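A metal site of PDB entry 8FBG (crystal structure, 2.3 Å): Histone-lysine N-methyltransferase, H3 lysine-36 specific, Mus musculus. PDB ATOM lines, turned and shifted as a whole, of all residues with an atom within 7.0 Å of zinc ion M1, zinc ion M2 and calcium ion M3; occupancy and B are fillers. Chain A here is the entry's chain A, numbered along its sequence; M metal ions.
The side-chain sulfur (SG) of Cys 45 binds calcium ion M3 (2.1 Å).
Calcium ion M3 is bound by the side-chain sulfur (SG) of Cys 70, 2.4 Å away.
SG of Cys 75 binds calcium ion M3, 2.6 Å away.
Calcium ion M3 has three donor atoms within binding distance.
Residues that only touch calcium ion M3: Asn 63 (3.96 Å).
Four residues have an atom within 4 Å of calcium ion M3: Cys 45, Asn 63, Cys 70 and Cys 75.
The nearest printed residue that does not touch calcium ion M3 is Cys 55 (4.1 Å).
Within 4 Å of zinc ion M1: Cys 55, Cys 70, Cys 75 and Cys 81.
The nearest printed residue that does not touch zinc ion M1 is Ala 77 (4.3 Å).
Zinc ion M1 is bound by the side-chain sulfur of Cys 81, the side-chain sulfur of Cys 75, the side-chain sulfur of Cys 55 and the side-chain sulfur of Cys 70.
Zinc ion M1 has four donor atoms within binding distance.
Within 4 Å of zinc ion M2: Cys 45, Cys 47, Cys 55, Cys 61 and Cys 70.
The backbone NH (N) of Cys 45 lies within hydrogen-bond range of the side-chain amide oxygen (OD1) of Asn 63.
The backbone carbonyl oxygen (O) of Cys 47 is in hydrogen-bond range of the backbone NH (N) of Ala 77, at 3.4 Å.
SG of Cys 81 sits close to NE2 of Gln 84 (3.2 Å).
The backbone NH of Ala 77 lies close to the side-chain sulfur of Cys 75 (3.6 Å).
O of Pro 43 sits at hydrogen-bond distance from ND2 of Asn 63, 2.9 Å away.
The side-chain amide nitrogen (ND2) of Asn 63 sits at hydrogen-bond distance from the backbone carbonyl oxygen (O) of Glu 69 (3.3 Å).
The backbone NH (N) of Cys 70 is in hydrogen-bond range of the backbone carbonyl oxygen (O) of Asn 83 (2.9 Å).
The backbone carbonyl oxygen (O) of Cys 55 is in hydrogen-bond range of the guanidinium group (NE) of Arg 64 (2.8 Å).
Zinc ion M2 is bound by the side-chain sulfur of Cys 61 (2.3 Å), the side-chain sulfur of Cys 55 (2.4 Å), the side-chain sulfur of Cys 47 (2.5 Å) and the side-chain sulfur of Cys 45 (2.5 Å).
Zinc ion M2 has four donor atoms within binding distance.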
ATOM      1  N   PRO A  43      10.474 -22.772   5.745  1.00  0.00           N
ATOM      2  CA  PRO A  43       9.514 -21.865   5.060  1.00  0.00           C
ATOM      3  C   PRO A  43      10.102 -20.469   4.774  1.00  0.00           C
ATOM      4  O   PRO A  43      11.123 -20.084   5.359  1.00  0.00           O
ATOM      5  CB  PRO A  43       8.330 -21.797   6.034  1.00  0.00           C
ATOM      6  CG  PRO A  43       8.843 -22.243   7.337  1.00  0.00           C
ATOM      7  CD  PRO A  43      10.011 -23.140   7.100  1.00  0.00           C
ATOM      8  N   ARG A  44       9.490 -19.737   3.848  1.00  0.00           N
ATOM      9  CA  ARG A  44       9.924 -18.394   3.443  1.00  0.00           C
ATOM     10  C   ARG A  44       8.804 -17.390   3.632  1.00  0.00           C
ATOM     11  O   ARG A  44       7.876 -17.362   2.834  1.00  0.00           O
ATOM     12  CB  ARG A  44      10.413 -18.390   1.973  1.00  0.00           C
ATOM     13  CG  ARG A  44      11.043 -17.051   1.529  1.00  0.00           C
ATOM     14  CD  ARG A  44      12.448 -16.814   2.093  1.00  0.00           C
ATOM     15  NE  ARG A  44      13.358 -17.896   1.688  1.00  0.00           N
ATOM     16  CZ  ARG A  44      14.020 -17.940   0.532  1.00  0.00           C
ATOM     17  NH1 ARG A  44      14.795 -18.980   0.244  1.00  0.00           N
ATOM     18  NH2 ARG A  44      13.925 -16.943  -0.332  1.00  0.00           N
ATOM     19  N   CYS A  45       8.925 -16.530   4.666  1.00  0.00           N
ATOM     20  CA  CYS A  45       7.934 -15.496   4.992  1.00  0.00           C
ATOM     21  C   CYS A  45       7.932 -14.402   3.944  1.00  0.00           C
ATOM     22  O   CYS A  45       8.780 -14.379   3.062  1.00  0.00           O
ATOM     23  CB  CYS A  45       8.178 -14.930   6.384  1.00  0.00           C
ATOM     24  SG  CYS A  45       9.587 -13.786   6.496  1.00  0.00           S
ATOM     25  N   ASN A  46       6.951 -13.501   4.052  1.00  0.00           N
ATOM     26  CA  ASN A  46       6.781 -12.389   3.137  1.00  0.00           C
ATOM     27  C   ASN A  46       6.599 -11.096   3.931  1.00  0.00           C
ATOM     28  O   ASN A  46       5.872 -10.196   3.518  1.00  0.00           O
ATOM     29  CB  ASN A  46       5.614 -12.657   2.159  1.00  0.00           C
ATOM     30  CG  ASN A  46       4.227 -12.747   2.775  1.00  0.00           C
ATOM     31  OD1 ASN A  46       4.036 -12.875   3.983  1.00  0.00           O
ATOM     32  ND2 ASN A  46       3.228 -12.684   1.925  1.00  0.00           N
ATOM     33  N   CYS A  47       7.281 -11.007   5.068  1.00  0.00           N
ATOM     34  CA  CYS A  47       7.294  -9.809   5.888  1.00  0.00           C
ATOM     35  C   CYS A  47       8.165  -8.795   5.164  1.00  0.00           C
ATOM     36  O   CYS A  47       9.110  -9.178   4.473  1.00  0.00           O
ATOM     37  CB  CYS A  47       7.829 -10.092   7.282  1.00  0.00           C
ATOM     38  SG  CYS A  47       6.855 -11.305   8.210  1.00  0.00           S
ATOM     39  N   LYS A  48       7.793  -7.520   5.275  1.00  0.00           N
ATOM     40  CA  LYS A  48       8.495  -6.445   4.636  1.00  0.00           C
ATOM     41  C   LYS A  48       9.285  -5.704   5.663  1.00  0.00           C
ATOM     42  O   LYS A  48       8.887  -5.671   6.840  1.00  0.00           O
ATOM     43  CB  LYS A  48       7.483  -5.491   3.945  1.00  0.00           C
ATOM     44  N   ASP A  51       7.274  -3.050   7.513  1.00  0.00           N
ATOM     45  CA  ASP A  51       6.255  -3.459   8.500  1.00  0.00           C
ATOM     46  C   ASP A  51       6.550  -2.886   9.890  1.00  0.00           C
ATOM     47  O   ASP A  51       7.706  -2.636  10.211  1.00  0.00           O
ATOM     48  CB  ASP A  51       6.167  -4.994   8.590  1.00  0.00           C
ATOM     49  CG  ASP A  51       5.531  -5.703   7.397  1.00  0.00           C
ATOM     50  OD1 ASP A  51       4.804  -5.053   6.616  1.00  0.00           O
ATOM     51  OD2 ASP A  51       5.740  -6.940   7.267  1.00  0.00           O
ATOM     52  N   PRO A  54       8.646  -6.300  11.794  1.00  0.00           N
ATOM     53  CA  PRO A  54       8.849  -7.380  10.787  1.00  0.00           C
ATOM     54  C   PRO A  54       9.318  -8.690  11.413  1.00  0.00           C
ATOM     55  O   PRO A  54      10.329  -8.737  12.126  1.00  0.00           O
ATOM     56  CB  PRO A  54       9.890  -6.779   9.839  1.00  0.00           C
ATOM     57  CG  PRO A  54       9.769  -5.295  10.017  1.00  0.00           C
ATOM     58  CD  PRO A  54       9.489  -5.125  11.480  1.00  0.00           C
ATOM     59  N   CYS A  55       8.491  -9.745  11.222  1.00  0.00           N
ATOM     60  CA  CYS A  55       8.675 -11.113  11.719  1.00  0.00           C
ATOM     61  C   CYS A  55       8.547 -11.207  13.247  1.00  0.00           C
ATOM     62  O   CYS A  55       8.864 -12.253  13.809  1.00  0.00           O
ATOM     63  CB  CYS A  55       9.994 -11.705  11.228  1.00  0.00           C
ATOM     64  SG  CYS A  55      10.330 -11.395   9.480  1.00  0.00           S
ATOM     65  N   GLY A  56       7.995 -10.175  13.886  1.00  0.00           N
ATOM     66  CA  GLY A  56       7.805 -10.079  15.334  1.00  0.00           C
ATOM     67  C   GLY A  56       6.661 -10.888  15.910  1.00  0.00           C
ATOM     68  O   GLY A  56       5.899 -11.501  15.161  1.00  0.00           O
ATOM     69  N   SER A  59       3.224 -10.404  14.281  1.00  0.00           N
ATOM     70  CA  SER A  59       3.174 -10.416  12.825  1.00  0.00           C
ATOM     71  C   SER A  59       2.547 -11.708  12.256  1.00  0.00           C
ATOM     72  O   SER A  59       2.213 -12.643  13.000  1.00  0.00           O
ATOM     73  CB  SER A  59       4.563 -10.196  12.217  1.00  0.00           C
ATOM     74  OG  SER A  59       5.400 -11.324  12.401  1.00  0.00           O
ATOM     75  N   GLU A  60       2.371 -11.726  10.934  1.00  0.00           N
ATOM     76  CA  GLU A  60       1.832 -12.841  10.181  1.00  0.00           C
ATOM     77  C   GLU A  60       2.987 -13.681   9.610  1.00  0.00           C
ATOM     78  O   GLU A  60       2.776 -14.386   8.615  1.00  0.00           O
ATOM     79  CB  GLU A  60       0.930 -12.311   9.053  1.00  0.00           C
ATOM     80  CG  GLU A  60      -0.313 -11.568   9.537  1.00  0.00           C
ATOM     81  CD  GLU A  60      -1.502 -12.458   9.815  1.00  0.00           C
ATOM     82  OE1 GLU A  60      -1.629 -12.946  10.964  1.00  0.00           O
ATOM     83  OE2 GLU A  60      -2.310 -12.666   8.878  1.00  0.00           O
ATOM     84  N   CYS A  61       4.198 -13.618  10.244  1.00  0.00           N
ATOM     85  CA  CYS A  61       5.416 -14.340   9.812  1.00  0.00           C
ATOM     86  C   CYS A  61       5.189 -15.845   9.834  1.00  0.00           C
ATOM     87  O   CYS A  61       5.064 -16.408  10.909  1.00  0.00           O
ATOM     88  CB  CYS A  61       6.628 -13.960  10.667  1.00  0.00           C
ATOM     89  SG  CYS A  61       8.204 -14.642  10.074  1.00  0.00           S
ATOM     90  N   ILE A  62       5.175 -16.485   8.655  1.00  0.00           N
ATOM     91  CA  ILE A  62       4.905 -17.922   8.543  1.00  0.00           C
ATOM     92  C   ILE A  62       5.996 -18.751   9.266  1.00  0.00           C
ATOM     93  O   ILE A  62       5.652 -19.746   9.900  1.00  0.00           O
ATOM     94  CB  ILE A  62       4.660 -18.393   7.096  1.00  0.00           C
ATOM     95  CG1 ILE A  62       4.386 -19.914   7.019  1.00  0.00           C
ATOM     96  CG2 ILE A  62       5.729 -17.964   6.112  1.00  0.00           C
ATOM     97  N   ASN A  63       7.257 -18.288   9.244  1.00  0.00           N
ATOM     98  CA  ASN A  63       8.374 -18.924   9.946  1.00  0.00           C
ATOM     99  C   ASN A  63       8.119 -18.929  11.470  1.00  0.00           C
ATOM    100  O   ASN A  63       8.177 -19.995  12.078  1.00  0.00           O
ATOM    101  CB  ASN A  63       9.701 -18.207   9.605  1.00  0.00           C
ATOM    102  CG  ASN A  63      10.208 -18.445   8.197  1.00  0.00           C
ATOM    103  OD1 ASN A  63       9.654 -17.956   7.213  1.00  0.00           O
ATOM    104  ND2 ASN A  63      11.281 -19.197   8.063  1.00  0.00           N
ATOM    105  N   ARG A  64       7.784 -17.743  12.070  1.00  0.00           N
ATOM    106  CA  ARG A  64       7.552 -17.630  13.520  1.00  0.00           C
ATOM    107  C   ARG A  64       6.400 -18.527  13.978  1.00  0.00           C
ATOM    108  O   ARG A  64       6.560 -19.227  14.974  1.00  0.00           O
ATOM    109  CB  ARG A  64       7.323 -16.160  13.925  1.00  0.00           C
ATOM    110  CG  ARG A  64       6.699 -15.967  15.315  1.00  0.00           C
ATOM    111  CD  ARG A  64       6.593 -14.502  15.687  1.00  0.00           C
ATOM    112  NE  ARG A  64       7.904 -13.883  15.849  1.00  0.00           N
ATOM    113  CZ  ARG A  64       8.593 -13.902  16.979  1.00  0.00           C
ATOM    114  NH1 ARG A  64       8.098 -14.502  18.054  1.00  0.00           N
ATOM    115  NH2 ARG A  64       9.795 -13.346  17.052  1.00  0.00           N
ATOM    116  N   GLU A  69      12.992 -20.042  12.806  1.00  0.00           N
ATOM    117  CA  GLU A  69      13.635 -18.752  12.774  1.00  0.00           C
ATOM    118  C   GLU A  69      13.711 -18.426  11.241  1.00  0.00           C
ATOM    119  O   GLU A  69      13.585 -19.338  10.402  1.00  0.00           O
ATOM    120  CB  GLU A  69      15.061 -18.906  13.296  1.00  0.00           C
ATOM    121  CG  GLU A  69      15.312 -18.428  14.717  1.00  0.00           C
ATOM    122  CD  GLU A  69      16.769 -18.083  14.925  1.00  0.00           C
ATOM    123  OE1 GLU A  69      17.518 -17.998  13.932  1.00  0.00           O
ATOM    124  OE2 GLU A  69      17.157 -17.878  16.102  1.00  0.00           O
ATOM    125  N   CYS A  70      13.949 -17.150  10.891  1.00  0.00           N
ATOM    126  CA  CYS A  70      14.176 -16.767   9.486  1.00  0.00           C
ATOM    127  C   CYS A  70      15.671 -16.942   9.195  1.00  0.00           C
ATOM    128  O   CYS A  70      16.500 -16.798  10.103  1.00  0.00           O
ATOM    129  CB  CYS A  70      13.741 -15.332   9.236  1.00  0.00           C
ATOM    130  SG  CYS A  70      11.964 -15.025   9.431  1.00  0.00           S
ATOM    131  N   HIS A  71      16.041 -17.228   7.931  1.00  0.00           N
ATOM    132  CA  HIS A  71      17.442 -17.311   7.502  1.00  0.00           C
ATOM    133  C   HIS A  71      17.852 -15.835   7.250  1.00  0.00           C
ATOM    134  O   HIS A  71      17.131 -15.145   6.520  1.00  0.00           O
ATOM    135  CB  HIS A  71      17.552 -18.197   6.250  1.00  0.00           C
ATOM    136  CG  HIS A  71      18.887 -18.238   5.577  1.00  0.00           C
ATOM    137  ND1 HIS A  71      19.720 -19.334   5.694  1.00  0.00           N
ATOM    138  CD2 HIS A  71      19.451 -17.368   4.709  1.00  0.00           C
ATOM    139  CE1 HIS A  71      20.787 -19.066   4.957  1.00  0.00           C
ATOM    140  NE2 HIS A  71      20.663 -17.895   4.341  1.00  0.00           N
ATOM    141  N   VAL A  74      18.172 -14.453   3.523  1.00  0.00           N
ATOM    142  CA  VAL A  74      17.056 -14.560   2.597  1.00  0.00           C
ATOM    143  C   VAL A  74      15.796 -13.903   3.173  1.00  0.00           C
ATOM    144  O   VAL A  74      14.844 -13.753   2.406  1.00  0.00           O
ATOM    145  CB  VAL A  74      16.735 -16.004   2.071  1.00  0.00           C
ATOM    146  CG1 VAL A  74      17.875 -16.576   1.258  1.00  0.00           C
ATOM    147  CG2 VAL A  74      16.319 -16.952   3.192  1.00  0.00           C
ATOM    148  N   CYS A  75      15.748 -13.526   4.487  1.00  0.00           N
ATOM    149  CA  CYS A  75      14.489 -12.914   4.983  1.00  0.00           C
ATOM    150  C   CYS A  75      14.217 -11.568   4.307  1.00  0.00           C
ATOM    151  O   CYS A  75      15.093 -10.689   4.376  1.00  0.00           O
ATOM    152  CB  CYS A  75      14.436 -12.783   6.496  1.00  0.00           C
ATOM    153  SG  CYS A  75      12.821 -12.205   7.102  1.00  0.00           S
ATOM    154  N   PRO A  76      13.026 -11.376   3.662  1.00  0.00           N
ATOM    155  CA  PRO A  76      12.776 -10.098   2.949  1.00  0.00           C
ATOM    156  C   PRO A  76      12.680  -8.889   3.875  1.00  0.00           C
ATOM    157  O   PRO A  76      12.809  -7.758   3.412  1.00  0.00           O
ATOM    158  CB  PRO A  76      11.450 -10.333   2.193  1.00  0.00           C
ATOM    159  CG  PRO A  76      11.104 -11.757   2.384  1.00  0.00           C
ATOM    160  CD  PRO A  76      11.885 -12.315   3.507  1.00  0.00           C
ATOM    161  N   ALA A  77      12.480  -9.133   5.184  1.00  0.00           N
ATOM    162  CA  ALA A  77      12.402  -8.076   6.191  1.00  0.00           C
ATOM    163  C   ALA A  77      13.812  -7.499   6.417  1.00  0.00           C
ATOM    164  O   ALA A  77      13.953  -6.413   6.993  1.00  0.00           O
ATOM    165  CB  ALA A  77      11.859  -8.638   7.493  1.00  0.00           C
ATOM    166  N   GLY A  78      14.814  -8.227   5.941  1.00  0.00           N
ATOM    167  CA  GLY A  78      16.219  -7.836   5.976  1.00  0.00           C
ATOM    168  C   GLY A  78      16.736  -7.640   7.385  1.00  0.00           C
ATOM    169  O   GLY A  78      16.297  -8.345   8.300  1.00  0.00           O
ATOM    170  N   ARG A  80      16.109  -5.683   9.786  1.00  0.00           N
ATOM    171  CA  ARG A  80      15.228  -5.491  10.927  1.00  0.00           C
ATOM    172  C   ARG A  80      14.252  -6.689  11.157  1.00  0.00           C
ATOM    173  O   ARG A  80      13.252  -6.531  11.868  1.00  0.00           O
ATOM    174  CB  ARG A  80      14.479  -4.146  10.879  1.00  0.00           C
ATOM    175  CG  ARG A  80      13.568  -3.856   9.709  1.00  0.00           C
ATOM    176  CD  ARG A  80      13.134  -2.391   9.823  1.00  0.00           C
ATOM    177  NE  ARG A  80      12.542  -2.088  11.147  1.00  0.00           N
ATOM    178  CZ  ARG A  80      11.257  -1.864  11.372  1.00  0.00           C
ATOM    179  NH1 ARG A  80      10.824  -1.615  12.604  1.00  0.00           N
ATOM    180  NH2 ARG A  80      10.392  -1.854  10.365  1.00  0.00           N
ATOM    181  N   CYS A  81      14.623  -7.891  10.660  1.00  0.00           N
ATOM    182  CA  CYS A  81      13.943  -9.166  10.922  1.00  0.00           C
ATOM    183  C   CYS A  81      13.945  -9.354  12.445  1.00  0.00           C
ATOM    184  O   CYS A  81      14.987  -9.177  13.072  1.00  0.00           O
ATOM    185  CB  CYS A  81      14.689 -10.310  10.234  1.00  0.00           C
ATOM    186  SG  CYS A  81      14.178 -11.967  10.764  1.00  0.00           S
ATOM    187  N   GLN A  82      12.793  -9.705  13.039  1.00  0.00           N
ATOM    188  CA  GLN A  82      12.692  -9.907  14.482  1.00  0.00           C
ATOM    189  C   GLN A  82      12.458 -11.385  14.819  1.00  0.00           C
ATOM    190  O   GLN A  82      11.919 -11.709  15.890  1.00  0.00           O
ATOM    191  CB  GLN A  82      11.572  -9.015  15.069  1.00  0.00           C
ATOM    192  CG  GLN A  82      11.862  -7.529  15.003  1.00  0.00           C
ATOM    193  CD  GLN A  82      10.750  -6.697  15.567  1.00  0.00           C
ATOM    194  OE1 GLN A  82       9.957  -7.150  16.404  1.00  0.00           O
ATOM    195  NE2 GLN A  82      10.672  -5.456  15.126  1.00  0.00           N
ATOM    196  N   ASN A  83      12.870 -12.271  13.925  1.00  0.00           N
ATOM    197  CA  ASN A  83      12.690 -13.719  14.118  1.00  0.00           C
ATOM    198  C   ASN A  83      14.043 -14.462  14.021  1.00  0.00           C
ATOM    199  O   ASN A  83      14.203 -15.423  13.243  1.00  0.00           O
ATOM    200  CB  ASN A  83      11.660 -14.269  13.150  1.00  0.00           C
ATOM    201  CG  ASN A  83      11.143 -15.646  13.481  1.00  0.00           C
ATOM    202  OD1 ASN A  83      11.132 -16.066  14.647  1.00  0.00           O
ATOM    203  ND2 ASN A  83      10.704 -16.374  12.449  1.00  0.00           N
ATOM    204  N   GLN A  84      15.006 -14.009  14.824  1.00  0.00           N
ATOM    205  CA  GLN A  84      16.348 -14.609  14.903  1.00  0.00           C
ATOM    206  C   GLN A  84      16.790 -14.658  16.373  1.00  0.00           C
ATOM    207  O   GLN A  84      17.977 -14.576  16.644  1.00  0.00           O
ATOM    208  CB  GLN A  84      17.365 -13.836  14.015  1.00  0.00           C
ATOM    209  CG  GLN A  84      17.132 -14.063  12.513  1.00  0.00           C
ATOM    210  CD  GLN A  84      17.853 -13.100  11.611  1.00  0.00           C
ATOM    211  OE1 GLN A  84      18.959 -12.644  11.882  1.00  0.00           O
ATOM    212  NE2 GLN A  84      17.237 -12.810  10.464  1.00  0.00           N
HETATM  213 ZN    ZN M   1      12.494 -12.420   9.333  1.00  0.00          ZN
HETATM  214 ZN    ZN M   2       8.696 -12.886   8.603  1.00  0.00          ZN
HETATM  215 CA    CA M   3      11.516 -14.468   7.095  1.00  0.00          CA
HETATM  216 CA    CA M   4      12.543 -16.102   5.795  1.00  0.00          CA
